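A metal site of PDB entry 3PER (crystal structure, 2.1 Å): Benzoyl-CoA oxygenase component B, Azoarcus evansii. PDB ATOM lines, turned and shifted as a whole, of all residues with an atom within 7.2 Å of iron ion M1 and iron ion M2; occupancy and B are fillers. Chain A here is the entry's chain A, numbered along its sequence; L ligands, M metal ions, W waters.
The side-chain carboxylate of Glu 120 is in hydrogen-bond range of the side-chain amide nitrogen of Gln 116. The backbone carbonyl oxygen (O) of Glu 120 sits at hydrogen-bond distance from the side-chain hydroxyl (OG) of Ser 123 (2.9 Å). A ring nitrogen (NE2) of His 243 sits at hydrogen-bond distance from the side-chain carboxylate of Glu 149 (2.7 Å). The backbone carbonyl oxygen (O) of Phe 206 sits at hydrogen-bond distance from the backbone NH (N) of Asp 211. NE2 of His 153 sits at hydrogen-bond distance from OE1 of Glu 239.
Within 4 Å of iron ion M1: Glu 120, Glu 150 and His 153. The nearest printed residue that does not touch iron ion M1 is Glu 240 (4.2 Å).
Four residues have an atom within 4 Å of iron ion M2: Glu 150, Asp 211, Glu 240 and His 243.
Iron ion M1 is bound by an oxygen (O1) of LIG L1 (1.9 Å). OE1 of Glu 120 binds iron ion M1 (2.0 Å). Iron ion M1 is bound by OE1 of Glu 150 (2.2 Å). Water W1 binds iron ion M1, at 2.2 Å. Iron ion M1 is bound by ND1 of His 153 (2.3 Å). An oxygen (O4) of LG2 L2 is bound to iron ion M1.
Iron ion M2 is bound by an oxygen (O2) of LG2 L2 (2.1 Å), the side-chain carboxylate of Glu 240 (2.2 Å), a ring nitrogen (ND1) of His 243 (2.2 Å), the side-chain carboxylate of Asp 211 (2.2 Å), an oxygen (O1) of LIG L1 (2.2 Å) and the side-chain carboxylate of Glu 150 (2.2 Å). Iron ion M2 has six donor atoms within binding distance.
Water W1 lies within hydrogen-bond range of OE2 of Glu 120 (2.5 Å), NE2 of Gln 116 (3.2 Å) and OE1 of Glu 240 (3.5 Å).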
ATOM      1  N   GLN A 116      14.397   4.915 -19.714  1.00  0.00           N
ATOM      2  CA  GLN A 116      13.654   3.661 -19.698  1.00  0.00           C
ATOM      3  C   GLN A 116      12.452   3.726 -20.683  1.00  0.00           C
ATOM      4  O   GLN A 116      12.194   2.779 -21.437  1.00  0.00           O
ATOM      5  CB  GLN A 116      13.177   3.350 -18.267  1.00  0.00           C
ATOM      6  CG  GLN A 116      12.273   2.139 -18.189  1.00  0.00           C
ATOM      7  CD  GLN A 116      12.992   0.870 -18.612  1.00  0.00           C
ATOM      8  OE1 GLN A 116      14.191   0.719 -18.375  1.00  0.00           O
ATOM      9  NE2 GLN A 116      12.264  -0.033 -19.256  1.00  0.00           N
ATOM     10  N   THR A 119      13.049   3.163 -24.637  1.00  0.00           N
ATOM     11  CA  THR A 119      13.325   1.852 -25.224  1.00  0.00           C
ATOM     12  C   THR A 119      12.038   1.162 -25.692  1.00  0.00           C
ATOM     13  O   THR A 119      12.087   0.268 -26.518  1.00  0.00           O
ATOM     14  CB  THR A 119      14.009   0.901 -24.197  1.00  0.00           C
ATOM     15  OG1 THR A 119      13.092   0.612 -23.135  1.00  0.00           O
ATOM     16  CG2 THR A 119      15.283   1.531 -23.642  1.00  0.00           C
ATOM     17  N   GLU A 120      10.906   1.557 -25.122  1.00  0.00           N
ATOM     18  CA  GLU A 120       9.651   0.838 -25.327  1.00  0.00           C
ATOM     19  C   GLU A 120       9.149   1.028 -26.784  1.00  0.00           C
ATOM     20  O   GLU A 120       9.050   0.062 -27.524  1.00  0.00           O
ATOM     21  CB  GLU A 120       8.608   1.279 -24.302  1.00  0.00           C
ATOM     22  CG  GLU A 120       9.135   1.366 -22.850  1.00  0.00           C
ATOM     23  CD  GLU A 120       9.514   0.006 -22.231  1.00  0.00           C
ATOM     24  OE1 GLU A 120       9.242  -1.032 -22.851  1.00  0.00           O
ATOM     25  OE2 GLU A 120      10.066  -0.020 -21.106  1.00  0.00           O
ATOM     26  N   SER A 123      11.558  -0.479 -29.461  1.00  0.00           N
ATOM     27  CA  SER A 123      11.463  -1.883 -29.833  1.00  0.00           C
ATOM     28  C   SER A 123      10.337  -2.119 -30.836  1.00  0.00           C
ATOM     29  O   SER A 123      10.440  -2.982 -31.700  1.00  0.00           O
ATOM     30  CB  SER A 123      11.234  -2.769 -28.608  1.00  0.00           C
ATOM     31  OG  SER A 123       9.904  -2.645 -28.117  1.00  0.00           O
ATOM     32  N   VAL A 146       3.711  -8.812 -27.787  1.00  0.00           N
ATOM     33  CA  VAL A 146       4.889  -8.099 -27.313  1.00  0.00           C
ATOM     34  C   VAL A 146       4.772  -6.643 -27.707  1.00  0.00           C
ATOM     35  O   VAL A 146       5.032  -5.759 -26.885  1.00  0.00           O
ATOM     36  CB  VAL A 146       6.209  -8.674 -27.884  1.00  0.00           C
ATOM     37  CG1 VAL A 146       7.394  -7.747 -27.537  1.00  0.00           C
ATOM     38  CG2 VAL A 146       6.479 -10.073 -27.311  1.00  0.00           C
ATOM     39  N   GLU A 149       2.243  -4.650 -25.590  1.00  0.00           N
ATOM     40  CA  GLU A 149       2.766  -4.507 -24.228  1.00  0.00           C
ATOM     41  C   GLU A 149       3.883  -3.449 -24.144  1.00  0.00           C
ATOM     42  O   GLU A 149       3.929  -2.671 -23.191  1.00  0.00           O
ATOM     43  CB  GLU A 149       3.247  -5.851 -23.691  1.00  0.00           C
ATOM     44  CG  GLU A 149       2.074  -6.777 -23.402  1.00  0.00           C
ATOM     45  CD  GLU A 149       2.495  -8.211 -23.186  1.00  0.00           C
ATOM     46  OE1 GLU A 149       3.679  -8.532 -23.342  1.00  0.00           O
ATOM     47  OE2 GLU A 149       1.622  -9.020 -22.880  1.00  0.00           O
ATOM     48  N   GLU A 150       4.776  -3.441 -25.134  1.00  0.00           N
ATOM     49  CA  GLU A 150       5.827  -2.421 -25.172  1.00  0.00           C
ATOM     50  C   GLU A 150       5.155  -1.055 -25.308  1.00  0.00           C
ATOM     51  O   GLU A 150       5.603  -0.073 -24.725  1.00  0.00           O
ATOM     52  CB  GLU A 150       6.807  -2.659 -26.322  1.00  0.00           C
ATOM     53  CG  GLU A 150       7.528  -4.009 -26.243  1.00  0.00           C
ATOM     54  CD  GLU A 150       8.387  -4.193 -24.966  1.00  0.00           C
ATOM     55  OE1 GLU A 150       8.173  -3.476 -23.964  1.00  0.00           O
ATOM     56  OE2 GLU A 150       9.283  -5.055 -24.976  1.00  0.00           O
ATOM     57  N   GLY A 151       4.066  -1.019 -26.079  1.00  0.00           N
ATOM     58  CA  GLY A 151       3.269   0.189 -26.181  1.00  0.00           C
ATOM     59  C   GLY A 151       2.738   0.607 -24.822  1.00  0.00           C
ATOM     60  O   GLY A 151       2.724   1.782 -24.506  1.00  0.00           O
ATOM     61  N   ARG A 152       2.297  -0.365 -24.012  1.00  0.00           N
ATOM     62  CA  ARG A 152       1.830  -0.054 -22.667  1.00  0.00           C
ATOM     63  C   ARG A 152       2.930   0.475 -21.779  1.00  0.00           C
ATOM     64  O   ARG A 152       2.674   1.292 -20.906  1.00  0.00           O
ATOM     65  CB  ARG A 152       1.172  -1.249 -21.963  1.00  0.00           C
ATOM     66  CG  ARG A 152       0.069  -0.777 -20.978  1.00  0.00           C
ATOM     67  CD  ARG A 152      -0.257  -1.816 -19.921  1.00  0.00           C
ATOM     68  NE  ARG A 152       0.926  -2.123 -19.113  1.00  0.00           N
ATOM     69  CZ  ARG A 152       1.393  -1.373 -18.114  1.00  0.00           C
ATOM     70  NH1 ARG A 152       2.480  -1.746 -17.456  1.00  0.00           N
ATOM     71  NH2 ARG A 152       0.760  -0.254 -17.767  1.00  0.00           N
ATOM     72  N   HIS A 153       4.160   0.009 -21.992  1.00  0.00           N
ATOM     73  CA  HIS A 153       5.255   0.436 -21.141  1.00  0.00           C
ATOM     74  C   HIS A 153       5.557   1.888 -21.413  1.00  0.00           C
ATOM     75  O   HIS A 153       5.979   2.618 -20.514  1.00  0.00           O
ATOM     76  CB  HIS A 153       6.489  -0.468 -21.331  1.00  0.00           C
ATOM     77  CG  HIS A 153       6.278  -1.840 -20.796  1.00  0.00           C
ATOM     78  ND1 HIS A 153       7.192  -2.863 -20.961  1.00  0.00           N
ATOM     79  CD2 HIS A 153       5.233  -2.372 -20.103  1.00  0.00           C
ATOM     80  CE1 HIS A 153       6.716  -3.961 -20.394  1.00  0.00           C
ATOM     81  NE2 HIS A 153       5.532  -3.698 -19.891  1.00  0.00           N
ATOM     82  N   LEU A 154       5.356   2.324 -22.662  1.00  0.00           N
ATOM     83  CA  LEU A 154       5.496   3.730 -22.976  1.00  0.00           C
ATOM     84  C   LEU A 154       4.438   4.495 -22.174  1.00  0.00           C
ATOM     85  O   LEU A 154       4.730   5.509 -21.562  1.00  0.00           O
ATOM     86  CB  LEU A 154       5.316   4.010 -24.470  1.00  0.00           C
ATOM     87  CG  LEU A 154       5.374   5.505 -24.784  1.00  0.00           C
ATOM     88  CD1 LEU A 154       6.671   6.112 -24.227  1.00  0.00           C
ATOM     89  CD2 LEU A 154       5.211   5.790 -26.275  1.00  0.00           C
ATOM     90  N   PHE A 206      16.553 -11.015 -29.416  1.00  0.00           N
ATOM     91  CA  PHE A 206      16.362  -9.711 -28.825  1.00  0.00           C
ATOM     92  C   PHE A 206      15.445  -9.813 -27.607  1.00  0.00           C
ATOM     93  O   PHE A 206      15.745  -9.240 -26.552  1.00  0.00           O
ATOM     94  CB  PHE A 206      15.789  -8.740 -29.862  1.00  0.00           C
ATOM     95  CG  PHE A 206      15.672  -7.317 -29.367  1.00  0.00           C
ATOM     96  CD1 PHE A 206      16.661  -6.378 -29.659  1.00  0.00           C
ATOM     97  CD2 PHE A 206      14.589  -6.921 -28.598  1.00  0.00           C
ATOM     98  CE1 PHE A 206      16.554  -5.058 -29.219  1.00  0.00           C
ATOM     99  CE2 PHE A 206      14.457  -5.609 -28.146  1.00  0.00           C
ATOM    100  CZ  PHE A 206      15.446  -4.676 -28.459  1.00  0.00           C
ATOM    101  N   THR A 207      14.357 -10.583 -27.732  1.00  0.00           N
ATOM    102  CA  THR A 207      13.408 -10.715 -26.631  1.00  0.00           C
ATOM    103  C   THR A 207      13.975 -11.647 -25.549  1.00  0.00           C
ATOM    104  O   THR A 207      13.625 -11.574 -24.367  1.00  0.00           O
ATOM    105  CB  THR A 207      11.980 -11.170 -27.101  1.00  0.00           C
ATOM    106  OG1 THR A 207      12.078 -12.319 -27.957  1.00  0.00           O
ATOM    107  CG2 THR A 207      11.280 -10.056 -27.886  1.00  0.00           C
ATOM    108  N   THR A 210      17.940  -8.869 -24.900  1.00  0.00           N
ATOM    109  CA  THR A 210      17.813  -7.430 -24.713  1.00  0.00           C
ATOM    110  C   THR A 210      16.604  -7.057 -23.849  1.00  0.00           C
ATOM    111  O   THR A 210      16.742  -6.192 -22.989  1.00  0.00           O
ATOM    112  CB  THR A 210      17.749  -6.727 -26.076  1.00  0.00           C
ATOM    113  OG1 THR A 210      18.819  -7.219 -26.877  1.00  0.00           O
ATOM    114  CG2 THR A 210      17.890  -5.217 -25.931  1.00  0.00           C
ATOM    115  N   ASP A 211      15.436  -7.668 -24.046  1.00  0.00           N
ATOM    116  CA  ASP A 211      14.332  -7.442 -23.102  1.00  0.00           C
ATOM    117  C   ASP A 211      14.776  -7.826 -21.694  1.00  0.00           C
ATOM    118  O   ASP A 211      14.198  -7.368 -20.704  1.00  0.00           O
ATOM    119  CB  ASP A 211      13.055  -8.223 -23.470  1.00  0.00           C
ATOM    120  CG  ASP A 211      12.281  -7.585 -24.647  1.00  0.00           C
ATOM    121  OD1 ASP A 211      12.944  -7.226 -25.637  1.00  0.00           O
ATOM    122  OD2 ASP A 211      11.037  -7.449 -24.585  1.00  0.00           O
ATOM    123  N   ARG A 212      15.793  -8.679 -21.585  1.00  0.00           N
ATOM    124  CA  ARG A 212      16.237  -9.102 -20.264  1.00  0.00           C
ATOM    125  C   ARG A 212      17.033  -7.987 -19.576  1.00  0.00           C
ATOM    126  O   ARG A 212      17.057  -7.904 -18.339  1.00  0.00           O
ATOM    127  CB  ARG A 212      17.085 -10.375 -20.327  1.00  0.00           C
ATOM    128  CG  ARG A 212      17.181 -11.099 -18.978  1.00  0.00           C
ATOM    129  CD  ARG A 212      17.928 -12.406 -19.135  1.00  0.00           C
ATOM    130  NE  ARG A 212      17.322 -13.249 -20.140  1.00  0.00           N
ATOM    131  CZ  ARG A 212      16.401 -14.182 -19.903  1.00  0.00           C
ATOM    132  NH1 ARG A 212      15.981 -14.430 -18.669  1.00  0.00           N
ATOM    133  NH2 ARG A 212      15.896 -14.882 -20.919  1.00  0.00           N
ATOM    134  N   GLY A 214      15.936  -5.069 -19.966  1.00  0.00           N
ATOM    135  CA  GLY A 214      14.756  -4.375 -19.457  1.00  0.00           C
ATOM    136  C   GLY A 214      14.385  -4.933 -18.084  1.00  0.00           C
ATOM    137  O   GLY A 214      14.151  -4.188 -17.140  1.00  0.00           O
ATOM    138  N   LYS A 215      14.339  -6.244 -17.986  1.00  0.00           N
ATOM    139  CA  LYS A 215      14.048  -6.899 -16.723  1.00  0.00           C
ATOM    140  C   LYS A 215      14.960  -6.388 -15.601  1.00  0.00           C
ATOM    141  O   LYS A 215      14.484  -5.982 -14.533  1.00  0.00           O
ATOM    142  CB  LYS A 215      14.201  -8.408 -16.864  1.00  0.00           C
ATOM    143  CG  LYS A 215      13.917  -9.187 -15.575  1.00  0.00           C
ATOM    144  CD  LYS A 215      14.523 -10.571 -15.649  1.00  0.00           C
ATOM    145  CE  LYS A 215      14.530 -11.259 -14.294  1.00  0.00           C
ATOM    146  NZ  LYS A 215      14.603 -12.735 -14.464  1.00  0.00           N
ATOM    147  N   LEU A 218      14.459  -2.656 -14.792  1.00  0.00           N
ATOM    148  CA  LEU A 218      13.163  -2.483 -14.120  1.00  0.00           C
ATOM    149  C   LEU A 218      13.211  -3.041 -12.691  1.00  0.00           C
ATOM    150  O   LEU A 218      12.578  -2.503 -11.800  1.00  0.00           O
ATOM    151  CB  LEU A 218      12.037  -3.178 -14.908  1.00  0.00           C
ATOM    152  CG  LEU A 218      11.651  -2.563 -16.268  1.00  0.00           C
ATOM    153  CD1 LEU A 218      10.643  -3.442 -17.035  1.00  0.00           C
ATOM    154  CD2 LEU A 218      11.110  -1.157 -16.048  1.00  0.00           C
ATOM    155  N   MET A 236       5.367  -4.029 -14.382  1.00  0.00           N
ATOM    156  CA  MET A 236       5.951  -4.267 -15.711  1.00  0.00           C
ATOM    157  C   MET A 236       6.818  -5.515 -15.740  1.00  0.00           C
ATOM    158  O   MET A 236       7.016  -6.101 -16.798  1.00  0.00           O
ATOM    159  CB  MET A 236       6.798  -3.069 -16.161  1.00  0.00           C
ATOM    160  CG  MET A 236       5.981  -1.851 -16.497  1.00  0.00           C
ATOM    161  SD  MET A 236       7.011  -0.373 -16.595  1.00  0.00           S
ATOM    162  CE  MET A 236       7.961  -0.774 -18.066  1.00  0.00           C
ATOM    163  N   GLU A 239       4.979  -8.449 -17.013  1.00  0.00           N
ATOM    164  CA  GLU A 239       4.817  -8.422 -18.468  1.00  0.00           C
ATOM    165  C   GLU A 239       6.128  -8.786 -19.169  1.00  0.00           C
ATOM    166  O   GLU A 239       6.147  -9.563 -20.120  1.00  0.00           O
ATOM    167  CB  GLU A 239       4.360  -7.047 -18.940  1.00  0.00           C
ATOM    168  CG  GLU A 239       2.999  -6.642 -18.383  1.00  0.00           C
ATOM    169  CD  GLU A 239       2.720  -5.159 -18.580  1.00  0.00           C
ATOM    170  OE1 GLU A 239       3.578  -4.331 -18.194  1.00  0.00           O
ATOM    171  OE2 GLU A 239       1.657  -4.829 -19.148  1.00  0.00           O
ATOM    172  N   GLU A 240       7.221  -8.226 -18.690  1.00  0.00           N
ATOM    173  CA  GLU A 240       8.542  -8.517 -19.246  1.00  0.00           C
ATOM    174  C   GLU A 240       8.809 -10.020 -19.252  1.00  0.00           C
ATOM    175  O   GLU A 240       9.505 -10.514 -20.120  1.00  0.00           O
ATOM    176  CB  GLU A 240       9.612  -7.800 -18.443  1.00  0.00           C
ATOM    177  CG  GLU A 240      10.972  -7.804 -19.101  1.00  0.00           C
ATOM    178  CD  GLU A 240      11.058  -6.855 -20.283  1.00  0.00           C
ATOM    179  OE1 GLU A 240      11.559  -5.710 -20.111  1.00  0.00           O
ATOM    180  OE2 GLU A 240      10.614  -7.242 -21.391  1.00  0.00           O
ATOM    181  N   ALA A 241       8.271 -10.741 -18.279  1.00  0.00           N
ATOM    182  CA  ALA A 241       8.427 -12.203 -18.223  1.00  0.00           C
ATOM    183  C   ALA A 241       7.889 -12.889 -19.480  1.00  0.00           C
ATOM    184  O   ALA A 241       8.460 -13.869 -19.972  1.00  0.00           O
ATOM    185  CB  ALA A 241       7.734 -12.775 -16.985  1.00  0.00           C
ATOM    186  N   HIS A 243       7.734 -11.597 -22.475  1.00  0.00           N
ATOM    187  CA  HIS A 243       8.646 -11.284 -23.581  1.00  0.00           C
ATOM    188  C   HIS A 243       9.837 -12.248 -23.581  1.00  0.00           C
ATOM    189  O   HIS A 243      10.255 -12.757 -24.626  1.00  0.00           O
ATOM    190  CB  HIS A 243       9.160  -9.847 -23.465  1.00  0.00           C
ATOM    191  CG  HIS A 243       8.082  -8.825 -23.466  1.00  0.00           C
ATOM    192  ND1 HIS A 243       8.333  -7.474 -23.387  1.00  0.00           N
ATOM    193  CD2 HIS A 243       6.730  -8.950 -23.526  1.00  0.00           C
ATOM    194  CE1 HIS A 243       7.190  -6.804 -23.393  1.00  0.00           C
ATOM    195  NE2 HIS A 243       6.197  -7.678 -23.468  1.00  0.00           N
ATOM    196  N   LEU A 244      10.364 -12.496 -22.387  1.00  0.00           N
ATOM    197  CA  LEU A 244      11.513 -13.364 -22.217  1.00  0.00           C
ATOM    198  C   LEU A 244      11.118 -14.775 -22.624  1.00  0.00           C
ATOM    199  O   LEU A 244      11.915 -15.510 -23.193  1.00  0.00           O
ATOM    200  CB  LEU A 244      11.971 -13.337 -20.774  1.00  0.00           C
ATOM    201  CG  LEU A 244      12.480 -11.983 -20.284  1.00  0.00           C
ATOM    202  CD1 LEU A 244      12.871 -12.091 -18.823  1.00  0.00           C
ATOM    203  CD2 LEU A 244      13.656 -11.483 -21.094  1.00  0.00           C
HETATM  204  O1  LIG L   1       9.282  -4.722 -21.614  1.00  0.00           O
HETATM  205  P1  LG2 L   2      12.203  -3.766 -23.523  1.00  0.00           P
HETATM  206  O1  LG2 L   2      12.265  -4.009 -25.024  1.00  0.00           O
HETATM  207  O2  LG2 L   2      11.728  -4.990 -22.794  1.00  0.00           O
HETATM  208  O3  LG2 L   2      13.574  -3.385 -23.044  1.00  0.00           O
HETATM  209  O4  LG2 L   2      11.229  -2.623 -23.293  1.00  0.00           O
HETATM  210 FE    FE M   1       9.186  -2.933 -22.104  1.00  0.00          FE
HETATM  211 FE    FE M   2      10.029  -6.148 -23.161  1.00  0.00          FE
HETATM  212  O   HOH W   1      10.499  -2.410 -20.374  1.00  0.00           O
